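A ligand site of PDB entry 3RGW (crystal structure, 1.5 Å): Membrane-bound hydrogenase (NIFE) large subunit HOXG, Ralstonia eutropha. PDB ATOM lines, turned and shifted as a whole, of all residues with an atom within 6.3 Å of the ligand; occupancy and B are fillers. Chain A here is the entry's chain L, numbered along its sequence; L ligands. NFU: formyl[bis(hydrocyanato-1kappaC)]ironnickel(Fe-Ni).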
ATOM      1  N   GLU A  27     -34.246   3.861  13.157  1.00  0.00           N
ATOM      2  CA  GLU A  27     -35.079   2.690  13.405  1.00  0.00           C
ATOM      3  C   GLU A  27     -34.926   2.265  14.855  1.00  0.00           C
ATOM      4  O   GLU A  27     -33.801   2.177  15.361  1.00  0.00           O
ATOM      5  CB  GLU A  27     -34.702   1.530  12.468  1.00  0.00           C
ATOM      6  CG  GLU A  27     -35.684   0.354  12.506  1.00  0.00           C
ATOM      7  CD  GLU A  27     -35.679  -0.365  13.852  1.00  0.00           C
ATOM      8  OE1 GLU A  27     -34.616  -0.391  14.501  1.00  0.00           O
ATOM      9  OE2 GLU A  27     -36.741  -0.922  14.243  1.00  0.00           O
ATOM     10  N   ILE A  74     -36.175  -9.368  12.749  1.00  0.00           N
ATOM     11  CA  ILE A  74     -35.290  -8.498  13.500  1.00  0.00           C
ATOM     12  C   ILE A  74     -35.450  -7.051  13.037  1.00  0.00           C
ATOM     13  O   ILE A  74     -35.401  -6.128  13.830  1.00  0.00           O
ATOM     14  CB  ILE A  74     -33.815  -8.942  13.396  1.00  0.00           C
ATOM     15  CG1 ILE A  74     -33.575 -10.173  14.257  1.00  0.00           C
ATOM     16  CG2 ILE A  74     -32.875  -7.805  13.841  1.00  0.00           C
ATOM     17  CD1 ILE A  74     -32.232 -10.826  14.045  1.00  0.00           C
ATOM     18  N   CYS A  75     -35.706  -6.864  11.740  1.00  0.00           N
ATOM     19  CA  CYS A  75     -35.770  -5.531  11.196  1.00  0.00           C
ATOM     20  C   CYS A  75     -36.536  -5.458   9.891  1.00  0.00           C
ATOM     21  O   CYS A  75     -36.258  -6.185   8.951  1.00  0.00           O
ATOM     22  CB  CYS A  75     -34.366  -4.980  11.004  1.00  0.00           C
ATOM     23  SG  CYS A  75     -34.324  -3.249  10.564  1.00  0.00           S
ATOM     24  N   GLY A  76     -37.451  -4.493   9.821  1.00  0.00           N
ATOM     25  CA  GLY A  76     -38.262  -4.288   8.638  1.00  0.00           C
ATOM     26  C   GLY A  76     -37.730  -3.198   7.738  1.00  0.00           C
ATOM     27  O   GLY A  76     -38.257  -2.959   6.662  1.00  0.00           O
ATOM     28  N   VAL A  77     -36.672  -2.523   8.194  1.00  0.00           N
ATOM     29  CA  VAL A  77     -35.979  -1.552   7.370  1.00  0.00           C
ATOM     30  C   VAL A  77     -34.904  -2.216   6.527  1.00  0.00           C
ATOM     31  O   VAL A  77     -34.954  -2.165   5.281  1.00  0.00           O
ATOM     32  CB  VAL A  77     -35.356  -0.442   8.236  1.00  0.00           C
ATOM     33  CG1 VAL A  77     -34.631   0.554   7.359  1.00  0.00           C
ATOM     34  CG2 VAL A  77     -36.445   0.263   9.051  1.00  0.00           C
ATOM     35  N   CYS A  78     -33.963  -2.901   7.183  1.00  0.00           N
ATOM     36  CA  CYS A  78     -33.045  -3.791   6.474  1.00  0.00           C
ATOM     37  C   CYS A  78     -33.690  -5.146   6.243  1.00  0.00           C
ATOM     38  O   CYS A  78     -33.144  -6.198   6.607  1.00  0.00           O
ATOM     39  CB  CYS A  78     -31.668  -3.898   7.192  1.00  0.00           C
ATOM     40  SG  CYS A  78     -31.675  -4.507   8.914  1.00  0.00           S
ATOM     41  N   THR A  79     -34.868  -5.123   5.637  1.00  0.00           N
ATOM     42  CA  THR A  79     -35.685  -6.304   5.515  1.00  0.00           C
ATOM     43  C   THR A  79     -35.103  -7.312   4.522  1.00  0.00           C
ATOM     44  O   THR A  79     -34.881  -6.989   3.347  1.00  0.00           O
ATOM     45  CB  THR A  79     -37.156  -5.941   5.132  1.00  0.00           C
ATOM     46  OG1 THR A  79     -37.915  -7.145   5.020  1.00  0.00           O
ATOM     47  CG2 THR A  79     -37.217  -5.185   3.817  1.00  0.00           C
ATOM     48  N   CYS A  81     -32.116  -8.858   4.899  1.00  0.00           N
ATOM     49  CA  CYS A  81     -30.686  -9.043   5.131  1.00  0.00           C
ATOM     50  C   CYS A  81     -30.437 -10.147   6.178  1.00  0.00           C
ATOM     51  O   CYS A  81     -29.489 -10.919   6.042  1.00  0.00           O
ATOM     52  CB  CYS A  81     -30.001  -7.714   5.530  1.00  0.00           C
ATOM     53  SG  CYS A  81     -30.164  -7.251   7.224  1.00  0.00           S
ATOM     54  N   HIS A  82     -31.326 -10.264   7.160  1.00  0.00           N
ATOM     55  CA  HIS A  82     -31.204 -11.298   8.178  1.00  0.00           C
ATOM     56  C   HIS A  82     -31.621 -12.659   7.635  1.00  0.00           C
ATOM     57  O   HIS A  82     -31.032 -13.675   7.984  1.00  0.00           O
ATOM     58  CB  HIS A  82     -32.012 -10.955   9.415  1.00  0.00           C
ATOM     59  CG  HIS A  82     -31.438  -9.831  10.198  1.00  0.00           C
ATOM     60  ND1 HIS A  82     -30.305  -9.965  10.983  1.00  0.00           N
ATOM     61  CD2 HIS A  82     -31.820  -8.538  10.303  1.00  0.00           C
ATOM     62  CE1 HIS A  82     -30.030  -8.797  11.538  1.00  0.00           C
ATOM     63  NE2 HIS A  82     -30.922  -7.917  11.146  1.00  0.00           N
ATOM     64  N   LEU A 113     -32.217  -4.007  -1.737  1.00  0.00           N
ATOM     65  CA  LEU A 113     -32.337  -3.539  -0.360  1.00  0.00           C
ATOM     66  C   LEU A 113     -31.350  -2.422  -0.085  1.00  0.00           C
ATOM     67  O   LEU A 113     -31.692  -1.426   0.543  1.00  0.00           O
ATOM     68  CB  LEU A 113     -32.132  -4.680   0.629  1.00  0.00           C
ATOM     69  CG  LEU A 113     -32.165  -4.264   2.103  1.00  0.00           C
ATOM     70  CD1 LEU A 113     -33.548  -3.732   2.486  1.00  0.00           C
ATOM     71  CD2 LEU A 113     -31.741  -5.418   3.009  1.00  0.00           C
ATOM     72  N   ASP A 117     -32.779   1.126   1.058  1.00  0.00           N
ATOM     73  CA  ASP A 117     -32.416   1.500   2.407  1.00  0.00           C
ATOM     74  C   ASP A 117     -31.600   2.802   2.403  1.00  0.00           C
ATOM     75  O   ASP A 117     -31.895   3.734   3.155  1.00  0.00           O
ATOM     76  CB  ASP A 117     -31.632   0.369   3.071  1.00  0.00           C
ATOM     77  CG  ASP A 117     -31.821   0.321   4.550  1.00  0.00           C
ATOM     78  OD1 ASP A 117     -31.902   1.397   5.173  1.00  0.00           O
ATOM     79  OD2 ASP A 117     -31.899  -0.804   5.109  1.00  0.00           O
ATOM     80  N   ALA A 528     -24.714  -6.047   4.961  1.00  0.00           N
ATOM     81  CA  ALA A 528     -25.980  -5.377   5.141  1.00  0.00           C
ATOM     82  C   ALA A 528     -25.809  -3.881   4.890  1.00  0.00           C
ATOM     83  O   ALA A 528     -24.690  -3.376   4.906  1.00  0.00           O
ATOM     84  CB  ALA A 528     -26.506  -5.628   6.542  1.00  0.00           C
ATOM     85  N   PRO A 529     -26.914  -3.171   4.666  1.00  0.00           N
ATOM     86  CA  PRO A 529     -26.821  -1.752   4.370  1.00  0.00           C
ATOM     87  C   PRO A 529     -25.985  -0.986   5.409  1.00  0.00           C
ATOM     88  O   PRO A 529     -25.261  -0.061   5.037  1.00  0.00           O
ATOM     89  CB  PRO A 529     -28.287  -1.296   4.390  1.00  0.00           C
ATOM     90  CG  PRO A 529     -29.036  -2.497   3.902  1.00  0.00           C
ATOM     91  CD  PRO A 529     -28.297  -3.687   4.496  1.00  0.00           C
ATOM     92  N   ARG A 530     -26.044  -1.390   6.676  1.00  0.00           N
ATOM     93  CA  ARG A 530     -25.376  -0.632   7.736  1.00  0.00           C
ATOM     94  C   ARG A 530     -23.994  -1.178   8.124  1.00  0.00           C
ATOM     95  O   ARG A 530     -23.315  -0.605   8.971  1.00  0.00           O
ATOM     96  CB  ARG A 530     -26.280  -0.499   8.958  1.00  0.00           C
ATOM     97  CG  ARG A 530     -27.442   0.444   8.732  1.00  0.00           C
ATOM     98  CD  ARG A 530     -28.623   0.143   9.619  1.00  0.00           C
ATOM     99  NE  ARG A 530     -29.758   0.971   9.246  1.00  0.00           N
ATOM    100  CZ  ARG A 530     -30.582   0.697   8.230  1.00  0.00           C
ATOM    101  NH1 ARG A 530     -30.430  -0.419   7.534  1.00  0.00           N
ATOM    102  NH2 ARG A 530     -31.559   1.536   7.924  1.00  0.00           N
ATOM    103  N   GLY A 531     -23.578  -2.259   7.470  1.00  0.00           N
ATOM    104  CA  GLY A 531     -22.235  -2.812   7.683  1.00  0.00           C
ATOM    105  C   GLY A 531     -22.208  -4.327   7.814  1.00  0.00           C
ATOM    106  O   GLY A 531     -22.976  -5.028   7.164  1.00  0.00           O
ATOM    107  N   ALA A 532     -21.327  -4.825   8.668  1.00  0.00           N
ATOM    108  CA  ALA A 532     -21.005  -6.246   8.709  1.00  0.00           C
ATOM    109  C   ALA A 532     -22.019  -7.013   9.549  1.00  0.00           C
ATOM    110  O   ALA A 532     -22.151  -6.775  10.748  1.00  0.00           O
ATOM    111  CB  ALA A 532     -19.601  -6.449   9.270  1.00  0.00           C
ATOM    112  N   LEU A 533     -22.731  -7.948   8.900  1.00  0.00           N
ATOM    113  CA  LEU A 533     -23.728  -8.785   9.573  1.00  0.00           C
ATOM    114  C   LEU A 533     -23.293 -10.247   9.583  1.00  0.00           C
ATOM    115  O   LEU A 533     -22.907 -10.781   8.561  1.00  0.00           O
ATOM    116  CB  LEU A 533     -25.090  -8.658   8.873  1.00  0.00           C
ATOM    117  CG  LEU A 533     -26.166  -9.665   9.294  1.00  0.00           C
ATOM    118  CD1 LEU A 533     -26.552  -9.452  10.748  1.00  0.00           C
ATOM    119  CD2 LEU A 533     -27.395  -9.560   8.373  1.00  0.00           C
ATOM    120  N   HIS A 535     -24.578 -14.242  11.215  1.00  0.00           N
ATOM    121  CA  HIS A 535     -25.376 -15.166  12.013  1.00  0.00           C
ATOM    122  C   HIS A 535     -24.569 -16.431  12.223  1.00  0.00           C
ATOM    123  O   HIS A 535     -24.085 -17.032  11.265  1.00  0.00           O
ATOM    124  CB  HIS A 535     -26.683 -15.538  11.289  1.00  0.00           C
ATOM    125  CG  HIS A 535     -27.696 -14.428  11.235  1.00  0.00           C
ATOM    126  ND1 HIS A 535     -29.036 -14.661  11.052  1.00  0.00           N
ATOM    127  CD2 HIS A 535     -27.561 -13.082  11.328  1.00  0.00           C
ATOM    128  CE1 HIS A 535     -29.691 -13.514  11.019  1.00  0.00           C
ATOM    129  NE2 HIS A 535     -28.815 -12.534  11.186  1.00  0.00           N
ATOM    130  N   VAL A 550     -24.625 -11.080  15.315  1.00  0.00           N
ATOM    131  CA  VAL A 550     -23.884  -9.856  15.547  1.00  0.00           C
ATOM    132  C   VAL A 550     -24.110  -8.935  14.368  1.00  0.00           C
ATOM    133  O   VAL A 550     -23.809  -9.295  13.230  1.00  0.00           O
ATOM    134  CB  VAL A 550     -22.376 -10.116  15.734  1.00  0.00           C
ATOM    135  CG1 VAL A 550     -21.665  -8.826  16.154  1.00  0.00           C
ATOM    136  CG2 VAL A 550     -22.149 -11.211  16.762  1.00  0.00           C
ATOM    137  N   VAL A 551     -24.714  -7.788  14.631  1.00  0.00           N
ATOM    138  CA  VAL A 551     -25.347  -7.001  13.591  1.00  0.00           C
ATOM    139  C   VAL A 551     -24.627  -5.637  13.463  1.00  0.00           C
ATOM    140  O   VAL A 551     -23.927  -5.234  14.369  1.00  0.00           O
ATOM    141  CB  VAL A 551     -26.847  -6.816  13.909  1.00  0.00           C
ATOM    142  CG1 VAL A 551     -27.566  -6.165  12.761  1.00  0.00           C
ATOM    143  CG2 VAL A 551     -27.471  -8.185  14.252  1.00  0.00           C
ATOM    144  N   PRO A 552     -24.733  -4.982  12.285  1.00  0.00           N
ATOM    145  CA  PRO A 552     -23.875  -3.819  12.079  1.00  0.00           C
ATOM    146  C   PRO A 552     -24.023  -2.765  13.188  1.00  0.00           C
ATOM    147  O   PRO A 552     -23.015  -2.255  13.682  1.00  0.00           O
ATOM    148  CB  PRO A 552     -24.351  -3.251  10.739  1.00  0.00           C
ATOM    149  CG  PRO A 552     -24.893  -4.449  10.006  1.00  0.00           C
ATOM    150  CD  PRO A 552     -25.433  -5.393  11.053  1.00  0.00           C
ATOM    151  N   THR A 553     -25.253  -2.442  13.562  1.00  0.00           N
ATOM    152  CA  THR A 553     -25.448  -1.427  14.591  1.00  0.00           C
ATOM    153  C   THR A 553     -25.069  -1.937  15.994  1.00  0.00           C
ATOM    154  O   THR A 553     -24.798  -1.135  16.883  1.00  0.00           O
ATOM    155  CB  THR A 553     -26.887  -0.859  14.562  1.00  0.00           C
ATOM    156  OG1 THR A 553     -27.149  -0.317  13.261  1.00  0.00           O
ATOM    157  CG2 THR A 553     -27.042   0.255  15.605  1.00  0.00           C
ATOM    158  N   THR A 554     -24.966  -3.260  16.157  1.00  0.00           N
ATOM    159  CA  THR A 554     -24.339  -3.804  17.364  1.00  0.00           C
ATOM    160  C   THR A 554     -22.889  -3.315  17.455  1.00  0.00           C
ATOM    161  O   THR A 554     -22.449  -2.886  18.504  1.00  0.00           O
ATOM    162  CB  THR A 554     -24.354  -5.350  17.409  1.00  0.00           C
ATOM    163  OG1 THR A 554     -25.638  -5.845  16.998  1.00  0.00           O
ATOM    164  CG2 THR A 554     -24.058  -5.841  18.815  1.00  0.00           C
ATOM    165  N   ASP A 595     -26.728   5.689  10.182  1.00  0.00           N
ATOM    166  CA  ASP A 595     -27.992   5.031   9.874  1.00  0.00           C
ATOM    167  C   ASP A 595     -28.329   4.002  10.982  1.00  0.00           C
ATOM    168  O   ASP A 595     -28.495   2.817  10.705  1.00  0.00           O
ATOM    169  CB  ASP A 595     -27.876   4.343   8.509  1.00  0.00           C
ATOM    170  CG  ASP A 595     -29.176   3.780   8.019  1.00  0.00           C
ATOM    171  OD1 ASP A 595     -30.229   4.031   8.645  1.00  0.00           O
ATOM    172  OD2 ASP A 595     -29.158   3.095   6.980  1.00  0.00           O
ATOM    173  N   PRO A 596     -28.432   4.465  12.242  1.00  0.00           N
ATOM    174  CA  PRO A 596     -28.589   3.531  13.362  1.00  0.00           C
ATOM    175  C   PRO A 596     -29.858   2.696  13.226  1.00  0.00           C
ATOM    176  O   PRO A 596     -30.938   3.239  12.982  1.00  0.00           O
ATOM    177  CB  PRO A 596     -28.695   4.458  14.582  1.00  0.00           C
ATOM    178  CG  PRO A 596     -28.017   5.722  14.158  1.00  0.00           C
ATOM    179  CD  PRO A 596     -28.347   5.862  12.700  1.00  0.00           C
ATOM    180  N   CYS A 597     -29.711   1.391  13.372  1.00  0.00           N
ATOM    181  CA  CYS A 597     -30.854   0.496  13.383  1.00  0.00           C
ATOM    182  C   CYS A 597     -30.893  -0.232  14.704  1.00  0.00           C
ATOM    183  O   CYS A 597     -30.155  -1.191  14.928  1.00  0.00           O
ATOM    184  CB  CYS A 597     -30.778  -0.495  12.236  1.00  0.00           C
ATOM    185  SG  CYS A 597     -32.308  -1.396  11.951  1.00  0.00           S
ATOM    186  N   LEU A 598     -31.723   0.258  15.626  1.00  0.00           N
ATOM    187  CA  LEU A 598     -31.635  -0.162  17.004  1.00  0.00           C
ATOM    188  C   LEU A 598     -32.295  -1.514  17.258  1.00  0.00           C
ATOM    189  O   LEU A 598     -31.829  -2.292  18.076  1.00  0.00           O
ATOM    190  CB  LEU A 598     -32.180   0.916  17.953  1.00  0.00           C
ATOM    191  CG  LEU A 598     -31.155   1.996  18.328  1.00  0.00           C
ATOM    192  CD1 LEU A 598     -30.091   1.433  19.255  1.00  0.00           C
ATOM    193  CD2 LEU A 598     -30.496   2.582  17.077  1.00  0.00           C
ATOM    194  N   ALA A 599     -33.370  -1.812  16.519  1.00  0.00           N
ATOM    195  CA  ALA A 599     -33.952  -3.143  16.553  1.00  0.00           C
ATOM    196  C   ALA A 599     -32.943  -4.181  16.066  1.00  0.00           C
ATOM    197  O   ALA A 599     -32.818  -5.267  16.633  1.00  0.00           O
ATOM    198  CB  ALA A 599     -35.218  -3.192  15.708  1.00  0.00           C
ATOM    199  N   CYS A 600     -32.204  -3.834  15.016  1.00  0.00           N
ATOM    200  CA  CYS A 600     -31.107  -4.677  14.555  1.00  0.00           C
ATOM    201  C   CYS A 600     -30.063  -4.868  15.647  1.00  0.00           C
ATOM    202  O   CYS A 600     -29.550  -5.976  15.847  1.00  0.00           O
ATOM    203  CB  CYS A 600     -30.446  -4.056  13.333  1.00  0.00           C
ATOM    204  SG  CYS A 600     -31.055  -4.683  11.744  1.00  0.00           S
ATOM    205  N   SER A 601     -29.691  -3.776  16.308  1.00  0.00           N
ATOM    206  CA  SER A 601     -28.536  -3.801  17.195  1.00  0.00           C
ATOM    207  C   SER A 601     -28.759  -4.738  18.372  1.00  0.00           C
ATOM    208  O   SER A 601     -27.817  -5.333  18.881  1.00  0.00           O
ATOM    209  CB  SER A 601     -28.203  -2.393  17.691  1.00  0.00           C
ATOM    210  OG  SER A 601     -29.160  -1.963  18.643  1.00  0.00           O
HETATM  211 FE   NFU L   1     -29.780  -4.013  10.024  1.00  0.00          FE
HETATM  212 NI   NFU L   1     -32.121  -2.995  10.467  1.00  0.00          NI
HETATM  213  C1  NFU L   1     -28.729  -5.574   9.788  1.00  0.00           C
HETATM  214  N1  NFU L   1     -28.063  -6.515   9.655  1.00  0.00           N
HETATM  215  C2  NFU L   1     -28.541  -3.220  11.118  1.00  0.00           C
HETATM  216  N2  NFU L   1     -27.738  -2.738  11.809  1.00  0.00           N
HETATM  217  C3  NFU L   1     -28.914  -3.282   8.498  1.00  0.00           C
HETATM  218  O3  NFU L   1     -28.371  -2.792   7.537  1.00  0.00           O
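FE of the ligand is bound by SG of Cys 600, 2.2 Å away.
The guanidinium group (NH1) of Arg 530 is in hydrogen-bond range of an oxygen (O3) of the ligand.
SG of Cys 597 binds NI of the ligand (2.2 Å).
N of Thr 553 is in hydrogen-bond range of N2 of the ligand.
The side-chain sulfur of Cys 78 binds a nickel atom (NI) of the ligand (2.2 Å).
N1 of the ligand lies within hydrogen-bond range of SG of Cys 81 (3.3 Å).
A nitrogen (N2) of the ligand sits at hydrogen-bond distance from the side-chain hydroxyl of Thr 553 (2.9 Å).
An oxygen (O3) of the ligand lies within hydrogen-bond range of the backbone NH (N) of Arg 530 (2.8 Å).
A nickel atom (NI) of the ligand is bound by the side-chain sulfur (SG) of Cys 75 (2.2 Å).
N of Pro 529 lies close to O3 of the ligand, at 3.2 Å.
His 82 touches the ligand (NE2 to C1, 3.5 Å).
Ala 528 touches the ligand.
Leu 533 touches the ligand.
Val 551 touches the ligand (CG1 to N1, 3.2 Å).
CD of Pro 552 touches N1 of the ligand (3.2 Å).
Hydrophobic or aromatic side chains that line the ligand: His 82, Ala 528, Pro 529, Leu 533, Val 551 and Pro 552.
Of the 30 residues printed, 13 come within 4 Å of the ligand.
A ring nitrogen (ND1) of His 82 is in hydrogen-bond range of a ring nitrogen (NE2) of His 535 (3.0 Å).
A ring nitrogen (NE2) of His 82 lies close to the side-chain sulfur (SG) of Cys 600 (3.3 Å).
The backbone carbonyl oxygen (O) of Val 551 lies close to the side-chain hydroxyl (OG1) of Thr 554 (3.2 Å).
The side-chain sulfur of Cys 597 lies close to the side-chain carboxylate of Glu 27, at 3.6 Å.
The backbone carbonyl oxygen of Cys 78 is in hydrogen-bond range of the side-chain sulfur of Cys 81.
NH2 of Arg 530 lies within salt-bridge range of OD1 of Asp 117.
OD1 of Asp 595 is in salt-bridge range of NH2 of Arg 530.
N of Cys 597 lies within hydrogen-bond range of OG1 of Thr 553.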
